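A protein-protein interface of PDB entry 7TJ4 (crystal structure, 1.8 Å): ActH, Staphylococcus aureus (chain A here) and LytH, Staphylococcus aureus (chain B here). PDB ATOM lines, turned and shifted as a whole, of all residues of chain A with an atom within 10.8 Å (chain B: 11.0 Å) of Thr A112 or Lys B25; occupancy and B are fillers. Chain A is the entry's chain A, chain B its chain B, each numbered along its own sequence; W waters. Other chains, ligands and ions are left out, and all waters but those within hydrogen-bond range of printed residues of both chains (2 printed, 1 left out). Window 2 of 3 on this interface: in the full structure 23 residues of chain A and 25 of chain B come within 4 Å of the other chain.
Water W2 bridges the side-chain hydroxyl (OG1) of Thr B148 and the backbone carbonyl oxygen (O) of Asp A113. Water W1 lies within hydrogen-bond range of N of Thr A112 (2.9 Å) and NZ of Lys B25 (3.5 Å).
Among the printed residues, pairs that only touch across the chains: Leu A117 with Thr B148, Asn A116 with Pro B147 and Asp A113 with Thr B151.
Thr A112 touches just one residue of chain B: Lys B25. Of chain B, only Tyr B26 (2.9 Å) and Thr B151 (3.7 Å) come within 4 Å of Asp A113. Ile A115 touches none of the printed residues of chain B. Asn A116 touches just one residue of chain B: Pro B147 (3.5 Å). Of the printed residues of chain B, Leu A117 touches Thr B148. No residue of chain A comes within 4 Å of Thr B24. Of chain A, only Thr A112 (3.0 Å) comes within 4 Å of Lys B25. Tyr B26 touches just one residue of chain A: Asp A113 (2.9 Å). Of the printed residues of chain A, Pro B147 touches Asn A116 (3.5 Å). Printed residues of chain A within 4 Å of Thr B148: Leu A117. The nearest residue of chain A that does not touch Lys B25 is Asp A113 (5.6 Å).
The side-chain carboxylate (OD1) of Asp A113 is in hydrogen-bond range of the side-chain hydroxyl (OH) of Tyr B26. OG1 of Thr A112 sits at hydrogen-bond distance from NZ of Lys B25, 3.0 Å away. The side-chain carboxylate (OE1) of Glu A120 sits at hydrogen-bond distance from the side-chain amide nitrogen (ND2) of Asn B146 (2.9 Å).
Hydrophobic or aromatic side chains of chain A within 4 Å of the printed part of chain B: Leu A117. Hydrophobic or aromatic side chains of chain B within 4 Å of the printed part of chain A: Tyr B26 and Pro B147. Among the printed residues, 6 pairs touch across the chains. Among the printed residues, no Asp or Glu carboxylate lies within 4 Å of a Lys or Arg side-chain nitrogen of the other chain.
The side-chain hydroxyl (OG1) of Thr B24 lies close to the backbone NH (N) of Tyr B26 (3.5 Å). The backbone carbonyl oxygen (O) of Thr B148 is in hydrogen-bond range of the side-chain hydroxyl (OG1) of Thr B151. The side-chain amide oxygen of Asn B146 lies close to the backbone NH of Thr B148, at 3.3 Å. The side-chain amide oxygen (OD1) of Asn A111 lies within hydrogen-bond range of the backbone NH (N) of Asp A113, at 2.9 Å. The backbone NH of Asp B149 lies within hydrogen-bond range of the side-chain amide oxygen of Asn B146, at 2.9 Å. The side-chain amide nitrogen of Asn A116 lies close to the backbone carbonyl oxygen of Thr A112, 3.3 Å away.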
ATOM      1  N   PHE A  82     -16.237  32.480   1.139  1.00  0.00           N
ATOM      2  CA  PHE A  82     -15.229  31.496   0.774  1.00  0.00           C
ATOM      3  C   PHE A  82     -15.126  31.387  -0.729  1.00  0.00           C
ATOM      4  O   PHE A  82     -14.019  31.381  -1.301  1.00  0.00           O
ATOM      5  CB  PHE A  82     -15.552  30.139   1.386  1.00  0.00           C
ATOM      6  CG  PHE A  82     -14.416  29.129   1.290  1.00  0.00           C
ATOM      7  CD1 PHE A  82     -13.183  29.410   1.833  1.00  0.00           C
ATOM      8  CD2 PHE A  82     -14.605  27.894   0.671  1.00  0.00           C
ATOM      9  CE1 PHE A  82     -12.127  28.452   1.741  1.00  0.00           C
ATOM     10  CE2 PHE A  82     -13.572  26.938   0.592  1.00  0.00           C
ATOM     11  CZ  PHE A  82     -12.331  27.216   1.117  1.00  0.00           C
ATOM     12  N   VAL A 101     -11.603  35.433   2.861  1.00  0.00           N
ATOM     13  CA  VAL A 101     -11.587  34.233   3.672  1.00  0.00           C
ATOM     14  C   VAL A 101     -11.650  34.592   5.138  1.00  0.00           C
ATOM     15  O   VAL A 101     -12.173  33.818   5.950  1.00  0.00           O
ATOM     16  CB  VAL A 101     -10.366  33.341   3.349  1.00  0.00           C
ATOM     17  CG1 VAL A 101      -9.061  33.940   3.828  1.00  0.00           C
ATOM     18  CG2 VAL A 101     -10.565  31.981   3.970  1.00  0.00           C
ATOM     19  N   ALA A 104     -15.138  34.878   5.943  1.00  0.00           N
ATOM     20  CA  ALA A 104     -15.759  33.564   6.081  1.00  0.00           C
ATOM     21  C   ALA A 104     -15.369  32.923   7.407  1.00  0.00           C
ATOM     22  O   ALA A 104     -16.170  32.204   8.016  1.00  0.00           O
ATOM     23  CB  ALA A 104     -15.387  32.660   4.896  1.00  0.00           C
ATOM     24  N   LEU A 105     -14.137  33.155   7.852  1.00  0.00           N
ATOM     25  CA  LEU A 105     -13.718  32.657   9.153  1.00  0.00           C
ATOM     26  C   LEU A 105     -14.456  33.357  10.284  1.00  0.00           C
ATOM     27  O   LEU A 105     -14.646  32.759  11.348  1.00  0.00           O
ATOM     28  CB  LEU A 105     -12.230  32.856   9.330  1.00  0.00           C
ATOM     29  CG  LEU A 105     -11.257  31.815   8.824  1.00  0.00           C
ATOM     30  CD1 LEU A 105      -9.891  32.452   8.855  1.00  0.00           C
ATOM     31  CD2 LEU A 105     -11.316  30.642   9.753  1.00  0.00           C
ATOM     32  N   ALA A 107     -17.546  33.999  10.216  1.00  0.00           N
ATOM     33  CA  ALA A 107     -18.790  33.241  10.320  1.00  0.00           C
ATOM     34  C   ALA A 107     -18.577  31.855  10.918  1.00  0.00           C
ATOM     35  O   ALA A 107     -19.514  31.257  11.451  1.00  0.00           O
ATOM     36  CB  ALA A 107     -19.438  33.109   8.933  1.00  0.00           C
ATOM     37  N   ASP A 108     -17.385  31.309  10.796  1.00  0.00           N
ATOM     38  CA  ASP A 108     -17.202  29.887  11.033  1.00  0.00           C
ATOM     39  C   ASP A 108     -15.725  29.677  11.334  1.00  0.00           C
ATOM     40  O   ASP A 108     -14.952  29.218  10.478  1.00  0.00           O
ATOM     41  CB  ASP A 108     -17.701  29.105   9.825  1.00  0.00           C
ATOM     42  CG  ASP A 108     -17.852  27.623  10.101  1.00  0.00           C
ATOM     43  OD1 ASP A 108     -17.635  27.230  11.273  1.00  0.00           O
ATOM     44  OD2 ASP A 108     -18.180  26.860   9.128  1.00  0.00           O
ATOM     45  N   PRO A 109     -15.293  30.059  12.539  1.00  0.00           N
ATOM     46  CA  PRO A 109     -13.855  30.053  12.857  1.00  0.00           C
ATOM     47  C   PRO A 109     -13.265  28.664  13.042  1.00  0.00           C
ATOM     48  O   PRO A 109     -12.027  28.541  13.064  1.00  0.00           O
ATOM     49  CB  PRO A 109     -13.780  30.876  14.158  1.00  0.00           C
ATOM     50  CG  PRO A 109     -15.144  30.825  14.728  1.00  0.00           C
ATOM     51  CD  PRO A 109     -16.087  30.736  13.568  1.00  0.00           C
ATOM     52  N   LYS A 110     -14.094  27.623  13.177  1.00  0.00           N
ATOM     53  CA  LYS A 110     -13.603  26.251  13.260  1.00  0.00           C
ATOM     54  C   LYS A 110     -13.596  25.518  11.918  1.00  0.00           C
ATOM     55  O   LYS A 110     -13.160  24.368  11.872  1.00  0.00           O
ATOM     56  CB  LYS A 110     -14.447  25.434  14.243  1.00  0.00           C
ATOM     57  CG  LYS A 110     -14.319  25.768  15.712  1.00  0.00           C
ATOM     58  CD  LYS A 110     -15.201  24.811  16.504  1.00  0.00           C
ATOM     59  CE  LYS A 110     -15.277  25.184  17.965  1.00  0.00           C
ATOM     60  NZ  LYS A 110     -13.979  24.945  18.651  1.00  0.00           N
ATOM     61  N   ASN A 111     -14.096  26.127  10.845  1.00  0.00           N
ATOM     62  CA  ASN A 111     -14.187  25.458   9.549  1.00  0.00           C
ATOM     63  C   ASN A 111     -12.785  25.180   8.995  1.00  0.00           C
ATOM     64  O   ASN A 111     -12.049  26.106   8.627  1.00  0.00           O
ATOM     65  CB  ASN A 111     -15.012  26.323   8.600  1.00  0.00           C
ATOM     66  CG  ASN A 111     -15.134  25.735   7.220  1.00  0.00           C
ATOM     67  OD1 ASN A 111     -14.142  25.440   6.559  1.00  0.00           O
ATOM     68  ND2 ASN A 111     -16.364  25.590   6.759  1.00  0.00           N
ATOM     69  N   THR A 112     -12.425  23.895   8.881  1.00  0.00           N
ATOM     70  CA  THR A 112     -11.048  23.555   8.499  1.00  0.00           C
ATOM     71  C   THR A 112     -10.707  23.973   7.054  1.00  0.00           C
ATOM     72  O   THR A 112      -9.548  24.291   6.769  1.00  0.00           O
ATOM     73  CB  THR A 112     -10.767  22.058   8.733  1.00  0.00           C
ATOM     74  OG1 THR A 112     -11.716  21.241   8.059  1.00  0.00           O
ATOM     75  CG2 THR A 112     -10.829  21.711  10.209  1.00  0.00           C
ATOM     76  N   ASP A 113     -11.686  24.050   6.149  1.00  0.00           N
ATOM     77  CA  ASP A 113     -11.384  24.576   4.814  1.00  0.00           C
ATOM     78  C   ASP A 113     -11.072  26.069   4.851  1.00  0.00           C
ATOM     79  O   ASP A 113     -10.108  26.513   4.217  1.00  0.00           O
ATOM     80  CB  ASP A 113     -12.531  24.325   3.841  1.00  0.00           C
ATOM     81  CG  ASP A 113     -12.909  22.872   3.728  1.00  0.00           C
ATOM     82  OD1 ASP A 113     -12.058  21.942   3.925  1.00  0.00           O
ATOM     83  OD2 ASP A 113     -14.079  22.659   3.383  1.00  0.00           O
ATOM     84  N   TYR A 114     -11.854  26.865   5.599  1.00  0.00           N
ATOM     85  CA  TYR A 114     -11.539  28.285   5.730  1.00  0.00           C
ATOM     86  C   TYR A 114     -10.176  28.477   6.380  1.00  0.00           C
ATOM     87  O   TYR A 114      -9.351  29.267   5.910  1.00  0.00           O
ATOM     88  CB  TYR A 114     -12.599  29.000   6.569  1.00  0.00           C
ATOM     89  CG  TYR A 114     -14.019  28.895   6.070  1.00  0.00           C
ATOM     90  CD1 TYR A 114     -14.309  28.379   4.809  1.00  0.00           C
ATOM     91  CD2 TYR A 114     -15.075  29.339   6.872  1.00  0.00           C
ATOM     92  CE1 TYR A 114     -15.635  28.292   4.358  1.00  0.00           C
ATOM     93  CE2 TYR A 114     -16.385  29.267   6.436  1.00  0.00           C
ATOM     94  CZ  TYR A 114     -16.662  28.734   5.174  1.00  0.00           C
ATOM     95  OH  TYR A 114     -17.973  28.669   4.740  1.00  0.00           O
ATOM     96  N   ILE A 115      -9.923  27.749   7.469  1.00  0.00           N
ATOM     97  CA  ILE A 115      -8.628  27.817   8.136  1.00  0.00           C
ATOM     98  C   ILE A 115      -7.492  27.483   7.177  1.00  0.00           C
ATOM     99  O   ILE A 115      -6.445  28.144   7.190  1.00  0.00           O
ATOM    100  CB  ILE A 115      -8.607  26.880   9.352  1.00  0.00           C
ATOM    101  CG1 ILE A 115      -9.548  27.376  10.442  1.00  0.00           C
ATOM    102  CG2 ILE A 115      -7.185  26.770   9.911  1.00  0.00           C
ATOM    103  CD1 ILE A 115     -10.080  26.259  11.264  1.00  0.00           C
ATOM    104  N   ASN A 116      -7.660  26.434   6.357  1.00  0.00           N
ATOM    105  CA  ASN A 116      -6.575  26.018   5.481  1.00  0.00           C
ATOM    106  C   ASN A 116      -6.251  27.103   4.469  1.00  0.00           C
ATOM    107  O   ASN A 116      -5.074  27.387   4.230  1.00  0.00           O
ATOM    108  CB  ASN A 116      -6.901  24.689   4.762  1.00  0.00           C
ATOM    109  CG  ASN A 116      -6.637  23.470   5.653  1.00  0.00           C
ATOM    110  OD1 ASN A 116      -5.862  23.562   6.605  1.00  0.00           O
ATOM    111  ND2 ASN A 116      -7.277  22.339   5.359  1.00  0.00           N
ATOM    112  N   LEU A 117      -7.283  27.742   3.879  1.00  0.00           N
ATOM    113  CA  LEU A 117      -7.014  28.737   2.846  1.00  0.00           C
ATOM    114  C   LEU A 117      -6.435  30.013   3.451  1.00  0.00           C
ATOM    115  O   LEU A 117      -5.549  30.653   2.871  1.00  0.00           O
ATOM    116  CB  LEU A 117      -8.293  29.026   2.058  1.00  0.00           C
ATOM    117  CG  LEU A 117      -8.192  30.129   0.989  1.00  0.00           C
ATOM    118  CD1 LEU A 117      -7.078  29.858  -0.035  1.00  0.00           C
ATOM    119  CD2 LEU A 117      -9.541  30.371   0.313  1.00  0.00           C
ATOM    120  N   GLU A 118      -6.920  30.410   4.618  1.00  0.00           N
ATOM    121  CA  GLU A 118      -6.332  31.581   5.243  1.00  0.00           C
ATOM    122  C   GLU A 118      -4.853  31.336   5.543  1.00  0.00           C
ATOM    123  O   GLU A 118      -4.004  32.192   5.269  1.00  0.00           O
ATOM    124  CB  GLU A 118      -7.121  31.925   6.495  1.00  0.00           C
ATOM    125  CG  GLU A 118      -6.617  33.120   7.245  1.00  0.00           C
ATOM    126  CD  GLU A 118      -5.957  32.693   8.529  1.00  0.00           C
ATOM    127  OE1 GLU A 118      -4.741  32.357   8.506  1.00  0.00           O
ATOM    128  OE2 GLU A 118      -6.667  32.659   9.560  1.00  0.00           O
ATOM    129  N   LYS A 119      -4.528  30.145   6.064  1.00  0.00           N
ATOM    130  CA  LYS A 119      -3.146  29.735   6.300  1.00  0.00           C
ATOM    131  C   LYS A 119      -2.325  29.825   5.020  1.00  0.00           C
ATOM    132  O   LYS A 119      -1.201  30.338   5.009  1.00  0.00           O
ATOM    133  CB  LYS A 119      -3.160  28.301   6.842  1.00  0.00           C
ATOM    134  CG  LYS A 119      -1.808  27.638   7.065  1.00  0.00           C
ATOM    135  CD  LYS A 119      -1.933  26.414   8.001  1.00  0.00           C
ATOM    136  CE  LYS A 119      -3.206  26.502   8.867  1.00  0.00           C
ATOM    137  NZ  LYS A 119      -3.081  25.825  10.224  1.00  0.00           N
ATOM    138  N   GLU A 120      -2.889  29.321   3.924  1.00  0.00           N
ATOM    139  CA  GLU A 120      -2.218  29.379   2.630  1.00  0.00           C
ATOM    140  C   GLU A 120      -1.888  30.811   2.239  1.00  0.00           C
ATOM    141  O   GLU A 120      -0.786  31.090   1.757  1.00  0.00           O
ATOM    142  CB  GLU A 120      -3.104  28.741   1.558  1.00  0.00           C
ATOM    143  CG  GLU A 120      -2.541  28.948   0.166  1.00  0.00           C
ATOM    144  CD  GLU A 120      -3.332  28.223  -0.918  1.00  0.00           C
ATOM    145  OE1 GLU A 120      -3.983  27.191  -0.625  1.00  0.00           O
ATOM    146  OE2 GLU A 120      -3.311  28.696  -2.075  1.00  0.00           O
ATOM    147  N   SER B  21      -2.443  11.454  -2.888  1.00  0.00           N
ATOM    148  CA  SER B  21      -3.496  11.540  -1.900  1.00  0.00           C
ATOM    149  C   SER B  21      -3.305  12.776  -1.012  1.00  0.00           C
ATOM    150  O   SER B  21      -2.185  13.214  -0.721  1.00  0.00           O
ATOM    151  CB  SER B  21      -3.565  10.249  -1.064  1.00  0.00           C
ATOM    152  OG  SER B  21      -2.287   9.953  -0.554  1.00  0.00           O
ATOM    153  N   SER B  22      -4.421  13.365  -0.627  1.00  0.00           N
ATOM    154  CA  SER B  22      -4.333  14.518   0.252  1.00  0.00           C
ATOM    155  C   SER B  22      -3.940  14.086   1.656  1.00  0.00           C
ATOM    156  O   SER B  22      -4.174  12.941   2.070  1.00  0.00           O
ATOM    157  CB  SER B  22      -5.676  15.228   0.299  1.00  0.00           C
ATOM    158  OG  SER B  22      -6.510  14.559   1.241  1.00  0.00           O
ATOM    159  N   ASN B  23      -3.368  15.043   2.403  1.00  0.00           N
ATOM    160  CA  ASN B  23      -3.030  14.909   3.824  1.00  0.00           C
ATOM    161  C   ASN B  23      -4.122  15.379   4.771  1.00  0.00           C
ATOM    162  O   ASN B  23      -3.903  15.370   5.994  1.00  0.00           O
ATOM    163  CB  ASN B  23      -1.781  15.722   4.163  1.00  0.00           C
ATOM    164  CG  ASN B  23      -0.555  15.309   3.344  1.00  0.00           C
ATOM    165  OD1 ASN B  23      -0.651  14.616   2.310  1.00  0.00           O
ATOM    166  ND2 ASN B  23       0.619  15.750   3.812  1.00  0.00           N
ATOM    167  N   THR B  24      -5.267  15.833   4.252  1.00  0.00           N
ATOM    168  CA  THR B  24      -6.311  16.383   5.107  1.00  0.00           C
ATOM    169  C   THR B  24      -7.176  15.254   5.666  1.00  0.00           C
ATOM    170  O   THR B  24      -7.006  14.072   5.337  1.00  0.00           O
ATOM    171  CB  THR B  24      -7.194  17.362   4.320  1.00  0.00           C
ATOM    172  OG1 THR B  24      -7.755  16.671   3.191  1.00  0.00           O
ATOM    173  CG2 THR B  24      -6.405  18.601   3.872  1.00  0.00           C
ATOM    174  N   LYS B  25      -8.173  15.645   6.467  1.00  0.00           N
ATOM    175  CA  LYS B  25      -9.117  14.701   7.049  1.00  0.00           C
ATOM    176  C   LYS B  25      -9.926  13.977   5.986  1.00  0.00           C
ATOM    177  O   LYS B  25     -10.459  12.905   6.260  1.00  0.00           O
ATOM    178  CB  LYS B  25     -10.032  15.456   8.005  1.00  0.00           C
ATOM    179  CG  LYS B  25     -10.842  16.515   7.281  1.00  0.00           C
ATOM    180  CD  LYS B  25     -11.595  17.416   8.240  1.00  0.00           C
ATOM    181  CE  LYS B  25     -12.925  17.843   7.637  1.00  0.00           C
ATOM    182  NZ  LYS B  25     -13.530  18.858   8.536  1.00  0.00           N
ATOM    183  N   TYR B  26     -10.002  14.526   4.765  1.00  0.00           N
ATOM    184  CA  TYR B  26     -10.751  13.900   3.683  1.00  0.00           C
ATOM    185  C   TYR B  26     -10.061  12.670   3.146  1.00  0.00           C
ATOM    186  O   TYR B  26     -10.737  11.784   2.625  1.00  0.00           O
ATOM    187  CB  TYR B  26     -10.960  14.885   2.528  1.00  0.00           C
ATOM    188  CG  TYR B  26     -11.643  16.134   3.006  1.00  0.00           C
ATOM    189  CD1 TYR B  26     -12.903  16.067   3.592  1.00  0.00           C
ATOM    190  CD2 TYR B  26     -11.022  17.371   2.918  1.00  0.00           C
ATOM    191  CE1 TYR B  26     -13.525  17.173   4.042  1.00  0.00           C
ATOM    192  CE2 TYR B  26     -11.663  18.504   3.386  1.00  0.00           C
ATOM    193  CZ  TYR B  26     -12.913  18.398   3.942  1.00  0.00           C
ATOM    194  OH  TYR B  26     -13.549  19.539   4.402  1.00  0.00           O
ATOM    195  N   LYS B  27      -8.739  12.615   3.262  1.00  0.00           N
ATOM    196  CA  LYS B  27      -7.898  11.558   2.697  1.00  0.00           C
ATOM    197  C   LYS B  27      -8.320  11.213   1.273  1.00  0.00           C
ATOM    198  O   LYS B  27      -8.604  10.066   0.935  1.00  0.00           O
ATOM    199  CB  LYS B  27      -7.916  10.320   3.599  1.00  0.00           C
ATOM    200  CG  LYS B  27      -7.388  10.536   5.034  1.00  0.00           C
ATOM    201  CD  LYS B  27      -5.986  11.142   5.030  1.00  0.00           C
ATOM    202  CE  LYS B  27      -5.362  11.089   6.426  1.00  0.00           C
ATOM    203  NZ  LYS B  27      -4.690   9.770   6.687  1.00  0.00           N
ATOM    204  N   SER B  28      -8.343  12.226   0.419  1.00  0.00           N
ATOM    205  CA  SER B  28      -8.801  12.017  -0.954  1.00  0.00           C
ATOM    206  C   SER B  28      -7.738  11.288  -1.780  1.00  0.00           C
ATOM    207  O   SER B  28      -6.543  11.547  -1.630  1.00  0.00           O
ATOM    208  CB  SER B  28      -9.155  13.359  -1.620  1.00  0.00           C
ATOM    209  OG  SER B  28     -10.103  14.108  -0.857  1.00  0.00           O
ATOM    210  N   LEU B  29      -8.194  10.396  -2.670  1.00  0.00           N
ATOM    211  CA  LEU B  29      -7.344   9.606  -3.556  1.00  0.00           C
ATOM    212  C   LEU B  29      -7.508  10.098  -4.979  1.00  0.00           C
ATOM    213  O   LEU B  29      -8.628  10.145  -5.497  1.00  0.00           O
ATOM    214  CB  LEU B  29      -7.689   8.119  -3.514  1.00  0.00           C
ATOM    215  CG  LEU B  29      -7.531   7.515  -2.120  1.00  0.00           C
ATOM    216  CD1 LEU B  29      -7.848   6.051  -2.204  1.00  0.00           C
ATOM    217  CD2 LEU B  29      -6.128   7.752  -1.489  1.00  0.00           C
ATOM    218  N   TYR B  33     -11.033  10.678  -8.054  1.00  0.00           N
ATOM    219  CA  TYR B  33     -11.516  11.929  -8.649  1.00  0.00           C
ATOM    220  C   TYR B  33     -11.202  12.070 -10.136  1.00  0.00           C
ATOM    221  O   TYR B  33     -12.010  12.682 -10.863  1.00  0.00           O
ATOM    222  CB  TYR B  33     -10.997  13.128  -7.852  1.00  0.00           C
ATOM    223  CG  TYR B  33     -11.675  13.075  -6.565  1.00  0.00           C
ATOM    224  CD1 TYR B  33     -13.019  13.501  -6.458  1.00  0.00           C
ATOM    225  CD2 TYR B  33     -11.074  12.467  -5.481  1.00  0.00           C
ATOM    226  CE1 TYR B  33     -13.703  13.386  -5.259  1.00  0.00           C
ATOM    227  CE2 TYR B  33     -11.743  12.366  -4.264  1.00  0.00           C
ATOM    228  CZ  TYR B  33     -13.057  12.813  -4.165  1.00  0.00           C
ATOM    229  OH  TYR B  33     -13.723  12.695  -2.977  1.00  0.00           O
ATOM    230  N   ILE B 144      -4.299  17.747  -5.658  1.00  0.00           N
ATOM    231  CA  ILE B 144      -4.963  17.150  -4.518  1.00  0.00           C
ATOM    232  C   ILE B 144      -4.205  17.423  -3.226  1.00  0.00           C
ATOM    233  O   ILE B 144      -4.791  17.340  -2.135  1.00  0.00           O
ATOM    234  CB  ILE B 144      -5.152  15.662  -4.775  1.00  0.00           C
ATOM    235  CG1 ILE B 144      -6.393  15.145  -4.052  1.00  0.00           C
ATOM    236  CG2 ILE B 144      -3.889  14.881  -4.413  1.00  0.00           C
ATOM    237  CD1 ILE B 144      -6.661  13.671  -4.492  1.00  0.00           C
ATOM    238  N   SER B 145      -2.940  17.814  -3.336  1.00  0.00           N
ATOM    239  CA  SER B 145      -2.099  18.230  -2.215  1.00  0.00           C
ATOM    240  C   SER B 145      -2.459  19.604  -1.672  1.00  0.00           C
ATOM    241  O   SER B 145      -2.036  19.948  -0.561  1.00  0.00           O
ATOM    242  CB  SER B 145      -0.635  18.251  -2.649  1.00  0.00           C
ATOM    243  OG  SER B 145      -0.489  19.059  -3.806  1.00  0.00           O
ATOM    244  N   ASN B 146      -3.210  20.390  -2.416  1.00  0.00           N
ATOM    245  CA  ASN B 146      -3.616  21.720  -1.956  1.00  0.00           C
ATOM    246  C   ASN B 146      -4.991  21.637  -1.296  1.00  0.00           C
ATOM    247  O   ASN B 146      -5.967  21.292  -1.973  1.00  0.00           O
ATOM    248  CB  ASN B 146      -3.654  22.702  -3.117  1.00  0.00           C
ATOM    249  CG  ASN B 146      -4.016  24.116  -2.672  1.00  0.00           C
ATOM    250  OD1 ASN B 146      -5.100  24.651  -3.008  1.00  0.00           O
ATOM    251  ND2 ASN B 146      -3.125  24.729  -1.901  1.00  0.00           N
ATOM    252  N   PRO B 147      -5.110  21.909   0.010  1.00  0.00           N
ATOM    253  CA  PRO B 147      -6.435  21.805   0.644  1.00  0.00           C
ATOM    254  C   PRO B 147      -7.529  22.518  -0.125  1.00  0.00           C
ATOM    255  O   PRO B 147      -8.587  21.931  -0.308  1.00  0.00           O
ATOM    256  CB  PRO B 147      -6.196  22.397   2.031  1.00  0.00           C
ATOM    257  CG  PRO B 147      -4.731  22.029   2.304  1.00  0.00           C
ATOM    258  CD  PRO B 147      -4.054  22.238   0.987  1.00  0.00           C
ATOM    259  N   THR B 148      -7.279  23.700  -0.687  1.00  0.00           N
ATOM    260  CA  THR B 148      -8.411  24.420  -1.282  1.00  0.00           C
ATOM    261  C   THR B 148      -8.762  23.881  -2.662  1.00  0.00           C
ATOM    262  O   THR B 148      -9.959  23.756  -3.003  1.00  0.00           O
ATOM    263  CB  THR B 148      -8.108  25.929  -1.303  1.00  0.00           C
ATOM    264  OG1 THR B 148      -7.912  26.368   0.039  1.00  0.00           O
ATOM    265  CG2 THR B 148      -9.281  26.731  -1.909  1.00  0.00           C
ATOM    266  N   ASP B 149      -7.754  23.521  -3.471  1.00  0.00           N
ATOM    267  CA  ASP B 149      -8.041  22.747  -4.685  1.00  0.00           C
ATOM    268  C   ASP B 149      -8.827  21.483  -4.358  1.00  0.00           C
ATOM    269  O   ASP B 149      -9.774  21.122  -5.064  1.00  0.00           O
ATOM    270  CB  ASP B 149      -6.743  22.345  -5.401  1.00  0.00           C
ATOM    271  CG  ASP B 149      -6.128  23.464  -6.228  1.00  0.00           C
ATOM    272  OD1 ASP B 149      -6.617  24.624  -6.232  1.00  0.00           O
ATOM    273  OD2 ASP B 149      -5.133  23.167  -6.930  1.00  0.00           O
ATOM    274  N   GLU B 150      -8.422  20.777  -3.311  1.00  0.00           N
ATOM    275  CA  GLU B 150      -9.086  19.537  -2.941  1.00  0.00           C
ATOM    276  C   GLU B 150     -10.579  19.768  -2.666  1.00  0.00           C
ATOM    277  O   GLU B 150     -11.422  18.966  -3.087  1.00  0.00           O
ATOM    278  CB  GLU B 150      -8.385  18.922  -1.723  1.00  0.00           C
ATOM    279  CG  GLU B 150      -9.068  17.660  -1.247  1.00  0.00           C
ATOM    280  CD  GLU B 150      -8.526  17.104   0.032  1.00  0.00           C
ATOM    281  OE1 GLU B 150      -7.935  17.863   0.828  1.00  0.00           O
ATOM    282  OE2 GLU B 150      -8.697  15.888   0.261  1.00  0.00           O
ATOM    283  N   THR B 151     -10.924  20.860  -1.974  1.00  0.00           N
ATOM    284  CA  THR B 151     -12.344  21.160  -1.783  1.00  0.00           C
ATOM    285  C   THR B 151     -13.057  21.277  -3.127  1.00  0.00           C
ATOM    286  O   THR B 151     -14.195  20.811  -3.264  1.00  0.00           O
ATOM    287  CB  THR B 151     -12.551  22.422  -0.913  1.00  0.00           C
ATOM    288  OG1 THR B 151     -12.371  23.640  -1.671  1.00  0.00           O
ATOM    289  CG2 THR B 151     -11.620  22.395   0.265  1.00  0.00           C
ATOM    290  N   LYS B 154     -13.240  17.613  -4.990  1.00  0.00           N
ATOM    291  CA  LYS B 154     -14.266  16.851  -4.308  1.00  0.00           C
ATOM    292  C   LYS B 154     -15.684  17.340  -4.631  1.00  0.00           C
ATOM    293  O   LYS B 154     -16.627  16.625  -4.318  1.00  0.00           O
ATOM    294  CB  LYS B 154     -14.060  16.960  -2.782  1.00  0.00           C
ATOM    295  CG  LYS B 154     -13.405  15.787  -2.098  1.00  0.00           C
ATOM    296  CD  LYS B 154     -13.697  15.866  -0.552  1.00  0.00           C
ATOM    297  CE  LYS B 154     -13.615  17.319  -0.020  1.00  0.00           C
ATOM    298  NZ  LYS B 154     -14.828  17.933   0.736  1.00  0.00           N
HETATM  299  O   HOH W   1     -14.597  22.072   9.233  1.00  0.00           O
HETATM  300  O   HOH W   2      -9.251  24.951   2.025  1.00  0.00           O
